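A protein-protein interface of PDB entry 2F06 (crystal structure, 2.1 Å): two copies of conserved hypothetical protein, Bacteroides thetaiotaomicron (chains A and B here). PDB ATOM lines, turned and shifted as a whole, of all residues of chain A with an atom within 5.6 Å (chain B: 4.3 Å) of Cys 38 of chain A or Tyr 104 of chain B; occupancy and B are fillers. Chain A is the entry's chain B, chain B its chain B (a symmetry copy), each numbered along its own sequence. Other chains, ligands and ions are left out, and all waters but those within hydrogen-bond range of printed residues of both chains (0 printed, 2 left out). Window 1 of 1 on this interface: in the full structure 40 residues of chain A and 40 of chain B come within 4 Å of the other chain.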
ATOM      1  N   ALA A  36       8.535 -23.951  20.769  1.00  0.00           N
ATOM      2  CA  ALA A  36       9.643 -24.450  19.943  1.00  0.00           C
ATOM      3  C   ALA A  36      10.266 -25.577  20.692  1.00  0.00           C
ATOM      4  O   ALA A  36      10.370 -25.563  21.943  1.00  0.00           O
ATOM      5  CB  ALA A  36      10.759 -23.367  19.688  1.00  0.00           C
ATOM      6  N   LEU A  37      10.729 -26.568  19.928  1.00  0.00           N
ATOM      7  CA  LEU A  37      11.491 -27.576  20.596  1.00  0.00           C
ATOM      8  C   LEU A  37      12.492 -28.197  19.642  1.00  0.00           C
ATOM      9  O   LEU A  37      12.404 -28.032  18.393  1.00  0.00           O
ATOM     10  CB  LEU A  37      10.578 -28.583  21.341  1.00  0.00           C
ATOM     11  CG  LEU A  37       9.693 -29.360  20.415  1.00  0.00           C
ATOM     12  CD1 LEU A  37      10.699 -30.249  19.635  1.00  0.00           C
ATOM     13  CD2 LEU A  37       8.615 -30.143  21.240  1.00  0.00           C
ATOM     14  N   CYS A  38      13.475 -28.848  20.237  1.00  0.00           N
ATOM     15  CA  CYS A  38      14.391 -29.635  19.448  1.00  0.00           C
ATOM     16  C   CYS A  38      15.025 -30.625  20.380  1.00  0.00           C
ATOM     17  O   CYS A  38      15.136 -30.425  21.595  1.00  0.00           O
ATOM     18  CB  CYS A  38      15.421 -28.771  18.727  1.00  0.00           C
ATOM     19  SG  CYS A  38      16.571 -28.086  19.820  1.00  0.00           S
ATOM     20  N   ILE A  39      15.331 -31.774  19.838  1.00  0.00           N
ATOM     21  CA  ILE A  39      15.949 -32.788  20.703  1.00  0.00           C
ATOM     22  C   ILE A  39      17.421 -32.922  20.322  1.00  0.00           C
ATOM     23  O   ILE A  39      17.759 -33.160  19.190  1.00  0.00           O
ATOM     24  CB  ILE A  39      15.250 -34.210  20.507  1.00  0.00           C
ATOM     25  CG1 ILE A  39      13.849 -34.177  21.115  1.00  0.00           C
ATOM     26  CG2 ILE A  39      16.115 -35.339  21.083  1.00  0.00           C
ATOM     27  CD1 ILE A  39      13.132 -35.527  21.035  1.00  0.00           C
ATOM     28  N   ALA A  40      18.296 -32.778  21.295  1.00  0.00           N
ATOM     29  CA  ALA A  40      19.725 -33.097  21.113  1.00  0.00           C
ATOM     30  C   ALA A  40      19.949 -34.521  21.659  1.00  0.00           C
ATOM     31  O   ALA A  40      19.920 -34.725  22.892  1.00  0.00           O
ATOM     32  CB  ALA A  40      20.573 -32.116  21.953  1.00  0.00           C
ATOM     33  N   ILE A  47      17.860 -35.299  24.978  1.00  0.00           N
ATOM     34  CA  ILE A  47      17.558 -34.113  25.741  1.00  0.00           C
ATOM     35  C   ILE A  47      16.593 -33.235  24.943  1.00  0.00           C
ATOM     36  O   ILE A  47      16.943 -32.775  23.851  1.00  0.00           O
ATOM     37  CB  ILE A  47      18.852 -33.323  25.896  1.00  0.00           C
ATOM     38  CG1 ILE A  47      19.979 -34.269  26.388  1.00  0.00           C
ATOM     39  CG2 ILE A  47      18.595 -32.042  26.780  1.00  0.00           C
ATOM     40  CD1 ILE A  47      19.695 -34.963  27.723  1.00  0.00           C
ATOM     41  N   LEU A  48      15.413 -33.013  25.472  1.00  0.00           N
ATOM     42  CA  LEU A  48      14.486 -32.133  24.877  1.00  0.00           C
ATOM     43  C   LEU A  48      14.822 -30.724  25.314  1.00  0.00           C
ATOM     44  O   LEU A  48      14.817 -30.454  26.492  1.00  0.00           O
ATOM     45  CB  LEU A  48      13.079 -32.462  25.342  1.00  0.00           C
ATOM     46  CG  LEU A  48      11.969 -31.697  24.619  1.00  0.00           C
ATOM     47  CD1 LEU A  48      11.865 -32.049  23.024  1.00  0.00           C
ATOM     48  CD2 LEU A  48      10.635 -32.073  25.315  1.00  0.00           C
ATOM     49  N   ARG A  49      15.040 -29.849  24.348  1.00  0.00           N
ATOM     50  CA  ARG A  49      15.230 -28.439  24.585  1.00  0.00           C
ATOM     51  C   ARG A  49      13.955 -27.796  24.139  1.00  0.00           C
ATOM     52  O   ARG A  49      13.558 -27.980  22.988  1.00  0.00           O
ATOM     53  CB  ARG A  49      16.379 -27.953  23.716  1.00  0.00           C
ATOM     54  CG  ARG A  49      17.699 -28.542  24.130  1.00  0.00           C
ATOM     55  CD  ARG A  49      18.846 -28.056  23.179  1.00  0.00           C
ATOM     56  NE  ARG A  49      20.135 -28.276  23.900  1.00  0.00           N
ATOM     57  CZ  ARG A  49      21.279 -28.421  23.239  1.00  0.00           C
ATOM     58  NH1 ARG A  49      21.285 -28.320  21.904  1.00  0.00           N
ATOM     59  NH2 ARG A  49      22.373 -28.620  23.885  1.00  0.00           N
ATOM     60  N   GLY A  50      13.322 -27.034  25.033  1.00  0.00           N
ATOM     61  CA  GLY A  50      11.980 -26.529  24.750  1.00  0.00           C
ATOM     62  C   GLY A  50      11.827 -25.073  25.158  1.00  0.00           C
ATOM     63  O   GLY A  50      12.373 -24.690  26.175  1.00  0.00           O
ATOM     64  N   TYR A 104      18.266 -23.047  17.002  1.00  0.00           N
ATOM     65  CA  TYR A 104      17.210 -23.743  16.306  1.00  0.00           C
ATOM     66  C   TYR A 104      16.271 -22.650  15.849  1.00  0.00           C
ATOM     67  O   TYR A 104      16.106 -21.599  16.517  1.00  0.00           O
ATOM     68  CB  TYR A 104      16.536 -24.900  17.107  1.00  0.00           C
ATOM     69  CG  TYR A 104      16.164 -24.620  18.627  1.00  0.00           C
ATOM     70  CD1 TYR A 104      17.142 -24.688  19.683  1.00  0.00           C
ATOM     71  CD2 TYR A 104      14.837 -24.358  18.981  1.00  0.00           C
ATOM     72  CE1 TYR A 104      16.766 -24.409  21.056  1.00  0.00           C
ATOM     73  CE2 TYR A 104      14.465 -24.103  20.341  1.00  0.00           C
ATOM     74  CZ  TYR A 104      15.435 -24.119  21.348  1.00  0.00           C
ATOM     75  OH  TYR A 104      15.033 -23.891  22.634  1.00  0.00           O
ATOM     76  N   SER A 105      15.709 -22.881  14.664  1.00  0.00           N
ATOM     77  CA  SER A 105      14.879 -21.883  13.947  1.00  0.00           C
ATOM     78  C   SER A 105      13.964 -22.574  12.951  1.00  0.00           C
ATOM     79  O   SER A 105      14.238 -23.666  12.539  1.00  0.00           O
ATOM     80  CB  SER A 105      15.723 -20.946  13.164  1.00  0.00           C
ATOM     81  OG  SER A 105      16.537 -21.653  12.301  1.00  0.00           O
ATOM     82  N   PHE A 106      12.839 -21.943  12.659  1.00  0.00           N
ATOM     83  CA  PHE A 106      11.894 -22.356  11.617  1.00  0.00           C
ATOM     84  C   PHE A 106      11.460 -21.050  11.015  1.00  0.00           C
ATOM     85  O   PHE A 106      11.360 -20.016  11.739  1.00  0.00           O
ATOM     86  CB  PHE A 106      10.628 -22.985  12.191  1.00  0.00           C
ATOM     87  CG  PHE A 106      10.508 -24.466  11.991  1.00  0.00           C
ATOM     88  CD1 PHE A 106      11.086 -25.350  12.915  1.00  0.00           C
ATOM     89  CD2 PHE A 106       9.765 -24.962  10.946  1.00  0.00           C
ATOM     90  CE1 PHE A 106      10.956 -26.679  12.786  1.00  0.00           C
ATOM     91  CE2 PHE A 106       9.651 -26.348  10.748  1.00  0.00           C
ATOM     92  CZ  PHE A 106      10.235 -27.206  11.688  1.00  0.00           C
ATOM     93  N   GLN B   8      16.836 -34.096   4.818  1.00  0.00           N
ATOM     94  CA  GLN B   8      17.452 -33.132   5.739  1.00  0.00           C
ATOM     95  C   GLN B   8      18.965 -33.103   5.449  1.00  0.00           C
ATOM     96  O   GLN B   8      19.619 -34.202   5.330  1.00  0.00           O
ATOM     97  CB  GLN B   8      17.238 -33.624   7.172  1.00  0.00           C
ATOM     98  CG  GLN B   8      17.842 -32.682   8.295  1.00  0.00           C
ATOM     99  CD  GLN B   8      17.866 -33.457   9.541  1.00  0.00           C
ATOM    100  OE1 GLN B   8      18.740 -34.334   9.764  1.00  0.00           O
ATOM    101  NE2 GLN B   8      16.849 -33.280  10.298  1.00  0.00           N
ATOM    102  N   ALA B  36      14.017 -24.565   8.157  1.00  0.00           N
ATOM    103  CA  ALA B  36      14.129 -24.991   9.558  1.00  0.00           C
ATOM    104  C   ALA B  36      15.544 -25.409   9.770  1.00  0.00           C
ATOM    105  O   ALA B  36      16.200 -25.999   8.877  1.00  0.00           O
ATOM    106  CB  ALA B  36      13.207 -26.222   9.905  1.00  0.00           C
ATOM    107  N   CYS B  38      18.427 -26.756  13.097  1.00  0.00           N
ATOM    108  CA  CYS B  38      18.780 -26.931  14.484  1.00  0.00           C
ATOM    109  C   CYS B  38      20.177 -27.480  14.510  1.00  0.00           C
ATOM    110  O   CYS B  38      20.658 -28.129  13.574  1.00  0.00           O
ATOM    111  CB  CYS B  38      17.789 -27.826  15.224  1.00  0.00           C
ATOM    112  SG  CYS B  38      17.916 -29.477  14.732  1.00  0.00           S
ATOM    113  N   GLY B  50      19.396 -29.189   8.686  1.00  0.00           N
ATOM    114  CA  GLY B  50      18.670 -28.127   7.994  1.00  0.00           C
ATOM    115  C   GLY B  50      17.638 -28.684   7.027  1.00  0.00           C
ATOM    116  O   GLY B  50      17.911 -29.687   6.396  1.00  0.00           O
ATOM    117  N   ILE B  51      16.454 -28.049   6.976  1.00  0.00           N
ATOM    118  CA  ILE B  51      15.526 -28.223   5.862  1.00  0.00           C
ATOM    119  C   ILE B  51      15.692 -26.976   5.008  1.00  0.00           C
ATOM    120  O   ILE B  51      15.585 -25.842   5.533  1.00  0.00           O
ATOM    121  CB  ILE B  51      14.034 -28.300   6.334  1.00  0.00           C
ATOM    122  CG1 ILE B  51      13.826 -29.422   7.340  1.00  0.00           C
ATOM    123  CG2 ILE B  51      13.107 -28.461   5.135  1.00  0.00           C
ATOM    124  CD1 ILE B  51      14.357 -30.886   6.892  1.00  0.00           C
ATOM    125  N   TYR B 102      15.135 -37.971  17.051  1.00  0.00           N
ATOM    126  CA  TYR B 102      15.093 -36.567  17.311  1.00  0.00           C
ATOM    127  C   TYR B 102      13.979 -35.919  16.569  1.00  0.00           C
ATOM    128  O   TYR B 102      13.394 -36.497  15.671  1.00  0.00           O
ATOM    129  CB  TYR B 102      16.428 -35.910  16.959  1.00  0.00           C
ATOM    130  CG  TYR B 102      16.896 -36.084  15.551  1.00  0.00           C
ATOM    131  CD1 TYR B 102      16.479 -35.182  14.555  1.00  0.00           C
ATOM    132  CD2 TYR B 102      17.786 -37.115  15.220  1.00  0.00           C
ATOM    133  CE1 TYR B 102      16.950 -35.278  13.259  1.00  0.00           C
ATOM    134  CE2 TYR B 102      18.285 -37.238  13.932  1.00  0.00           C
ATOM    135  CZ  TYR B 102      17.862 -36.298  12.970  1.00  0.00           C
ATOM    136  OH  TYR B 102      18.301 -36.394  11.688  1.00  0.00           O
ATOM    137  N   MET B 103      13.661 -34.703  16.944  1.00  0.00           N
ATOM    138  CA  MET B 103      12.662 -33.938  16.222  1.00  0.00           C
ATOM    139  C   MET B 103      12.941 -32.487  16.536  1.00  0.00           C
ATOM    140  O   MET B 103      13.715 -32.179  17.508  1.00  0.00           O
ATOM    141  CB  MET B 103      11.237 -34.316  16.695  1.00  0.00           C
ATOM    142  CG  MET B 103      10.921 -33.922  18.135  1.00  0.00           C
ATOM    143  SD  MET B 103       9.023 -34.350  18.440  1.00  0.00           S
ATOM    144  CE  MET B 103       8.582 -32.411  18.234  1.00  0.00           C
ATOM    145  N   TYR B 104      12.377 -31.601  15.739  1.00  0.00           N
ATOM    146  CA  TYR B 104      12.479 -30.184  15.985  1.00  0.00           C
ATOM    147  C   TYR B 104      11.212 -29.604  15.402  1.00  0.00           C
ATOM    148  O   TYR B 104      10.656 -30.109  14.394  1.00  0.00           O
ATOM    149  CB  TYR B 104      13.800 -29.516  15.488  1.00  0.00           C
ATOM    150  CG  TYR B 104      14.320 -29.908  14.038  1.00  0.00           C
ATOM    151  CD1 TYR B 104      15.041 -31.129  13.783  1.00  0.00           C
ATOM    152  CD2 TYR B 104      14.133 -29.024  12.971  1.00  0.00           C
ATOM    153  CE1 TYR B 104      15.483 -31.458  12.442  1.00  0.00           C
ATOM    154  CE2 TYR B 104      14.590 -29.343  11.651  1.00  0.00           C
ATOM    155  CZ  TYR B 104      15.241 -30.556  11.408  1.00  0.00           C
ATOM    156  OH  TYR B 104      15.679 -30.811  10.139  1.00  0.00           O
ATOM    157  N   SER B 105      10.721 -28.575  16.090  1.00  0.00           N
ATOM    158  CA  SER B 105       9.408 -27.949  15.797  1.00  0.00           C
ATOM    159  C   SER B 105       9.365 -26.532  16.342  1.00  0.00           C
ATOM    160  O   SER B 105      10.101 -26.205  17.230  1.00  0.00           O
ATOM    161  CB  SER B 105       8.302 -28.687  16.456  1.00  0.00           C
ATOM    162  OG  SER B 105       8.539 -28.776  17.814  1.00  0.00           O
ATOM    163  N   ASN B 113       4.746 -26.918  12.919  1.00  0.00           N
ATOM    164  CA  ASN B 113       5.423 -27.841  11.937  1.00  0.00           C
ATOM    165  C   ASN B 113       6.517 -28.514  12.674  1.00  0.00           C
ATOM    166  O   ASN B 113       7.241 -27.873  13.464  1.00  0.00           O
ATOM    167  CB  ASN B 113       6.034 -27.121  10.757  1.00  0.00           C
ATOM    168  CG  ASN B 113       4.993 -26.372   9.966  1.00  0.00           C
ATOM    169  OD1 ASN B 113       4.951 -25.138  10.022  1.00  0.00           O
ATOM    170  ND2 ASN B 113       4.100 -27.078   9.343  1.00  0.00           N
ATOM    171  N   VAL B 114       6.555 -29.824  12.518  1.00  0.00           N
ATOM    172  CA  VAL B 114       7.458 -30.672  13.302  1.00  0.00           C
ATOM    173  C   VAL B 114       8.203 -31.546  12.301  1.00  0.00           C
ATOM    174  O   VAL B 114       7.571 -32.212  11.467  1.00  0.00           O
ATOM    175  CB  VAL B 114       6.658 -31.624  14.282  1.00  0.00           C
ATOM    176  CG1 VAL B 114       7.641 -32.431  15.155  1.00  0.00           C
ATOM    177  CG2 VAL B 114       5.722 -30.794  15.196  1.00  0.00           C
ATOM    178  N   VAL B 115       9.511 -31.540  12.423  1.00  0.00           N
ATOM    179  CA  VAL B 115      10.362 -32.455  11.679  1.00  0.00           C
ATOM    180  C   VAL B 115      10.760 -33.631  12.598  1.00  0.00           C
ATOM    181  O   VAL B 115      11.284 -33.412  13.658  1.00  0.00           O
ATOM    182  CB  VAL B 115      11.592 -31.701  11.035  1.00  0.00           C
ATOM    183  CG1 VAL B 115      12.490 -32.716  10.298  1.00  0.00           C
ATOM    184  CG2 VAL B 115      11.088 -30.564  10.080  1.00  0.00           C
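Printed residues of chain A that touch a printed residue of chain B: Ala 36, Leu 37, Cys 38, Ile 39, Tyr 104, Ser 105 and Phe 106.
Hydrophobic or aromatic side chains of chain A within 4 Å of the printed part of chain B: Ala 36, Leu 37, Ile 39, Tyr 104 and Phe 106.
Of the 12 printed residues of chain B, 8 touch a printed residue of chain A.
O of Met 103 of chain B lies within hydrogen-bond range of N of Ile 39 of chain A, at 2.9 Å.
The backbone NH (N) of Leu 37 of chain A is in hydrogen-bond range of the backbone carbonyl oxygen (O) of Ser 105 of chain B, 2.8 Å away.
The side-chain amide nitrogen of Gln 8 of chain B is in hydrogen-bond range of the side-chain hydroxyl of Tyr 104 of chain B.
O of Cys 38 of chain A lies within hydrogen-bond range of N of Arg 49 of chain A, 2.8 Å away.
O of Ala 36 of chain B lies within hydrogen-bond range of N of Ile 51 of chain B (2.8 Å).
The backbone NH of Val 115 of chain B lies within hydrogen-bond range of the backbone carbonyl oxygen of Tyr 104 of chain B, at 2.7 Å.
The side-chain amide oxygen of Gln 8 of chain B lies within hydrogen-bond range of the side-chain hydroxyl of Tyr 102 of chain B (2.9 Å).
Ala 36 of chain A touches Ser 105 of chain B, and with the chains exchanged Ser 105 of chain A touches Ala 36 of chain B.
Cys 38 of chain A touches Tyr 104 of chain B, and with the chains exchanged Tyr 104 of chain A touches Cys 38 of chain B.
Positions printed for both chains: 36, 38, 50, 104 and 105.
Printed residues of chain B within 4 Å of Cys 38 of chain A: Met 103 (3.3 Å) and Tyr 104 (3.7 Å).
Of the printed residues of chain A, Tyr 104 of chain B touches Leu 37, Cys 38 and Phe 106.
Printed residues of chain A within 4 Å of Tyr 102 of chain B: Ile 39 (3.8 Å).
Of the printed residues of chain B, Phe 106 of chain A touches Ala 36 (3.6 Å), Tyr 104 (3.8 Å), Ser 105 (3.6 Å), Asn 113 (3.5 Å) and Val 115 (3.8 Å).
Printed residues of chain B within 4 Å of Ile 39 of chain A: Tyr 102 (3.8 Å) and Met 103 (2.9 Å).
Printed residues of chain A within 4 Å of Val 115 of chain B: Phe 106 (3.8 Å).
Printed residues of chain A within 4 Å of Ser 105 of chain B: Ala 36, Leu 37 and Phe 106.
Gln 8 of chain B touches none of the printed residues of chain A.
Arg 49 of chain A touches none of the printed residues of chain B.
The nearest printed residue of chain B that does not touch Cys 38 of chain A is Cys 38 of chain B (4.3 Å).
The nearest printed residue of chain B that does not touch Leu 37 of chain A is Val 114 of chain B (5.8 Å).
Among the printed residues, merely in contact across the chains: Ala 36 of chain A with Ser 105 of chain B (3.3 Å), Leu 37 of chain A with Met 103 of chain B (3.3 Å), Leu 37 of chain A with Tyr 104 of chain B (3.2 Å), Cys 38 of chain A with Met 103 of chain B (3.3 Å), Cys 38 of chain A with Tyr 104 of chain B (3.7 Å), Ile 39 of chain A with Tyr 102 of chain B (3.8 Å), Tyr 104 of chain A with Cys 38 of chain B (3.7 Å), Ser 105 of chain A with Ala 36 of chain B (3.3 Å), Phe 106 of chain A with Ala 36 of chain B (3.6 Å), Phe 106 of chain A with Tyr 104 of chain B (3.8 Å), Phe 106 of chain A with Ser 105 of chain B (3.6 Å), Phe 106 of chain A with Asn 113 of chain B (3.5 Å) and Phe 106 of chain A with Val 115 of chain B (3.8 Å).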
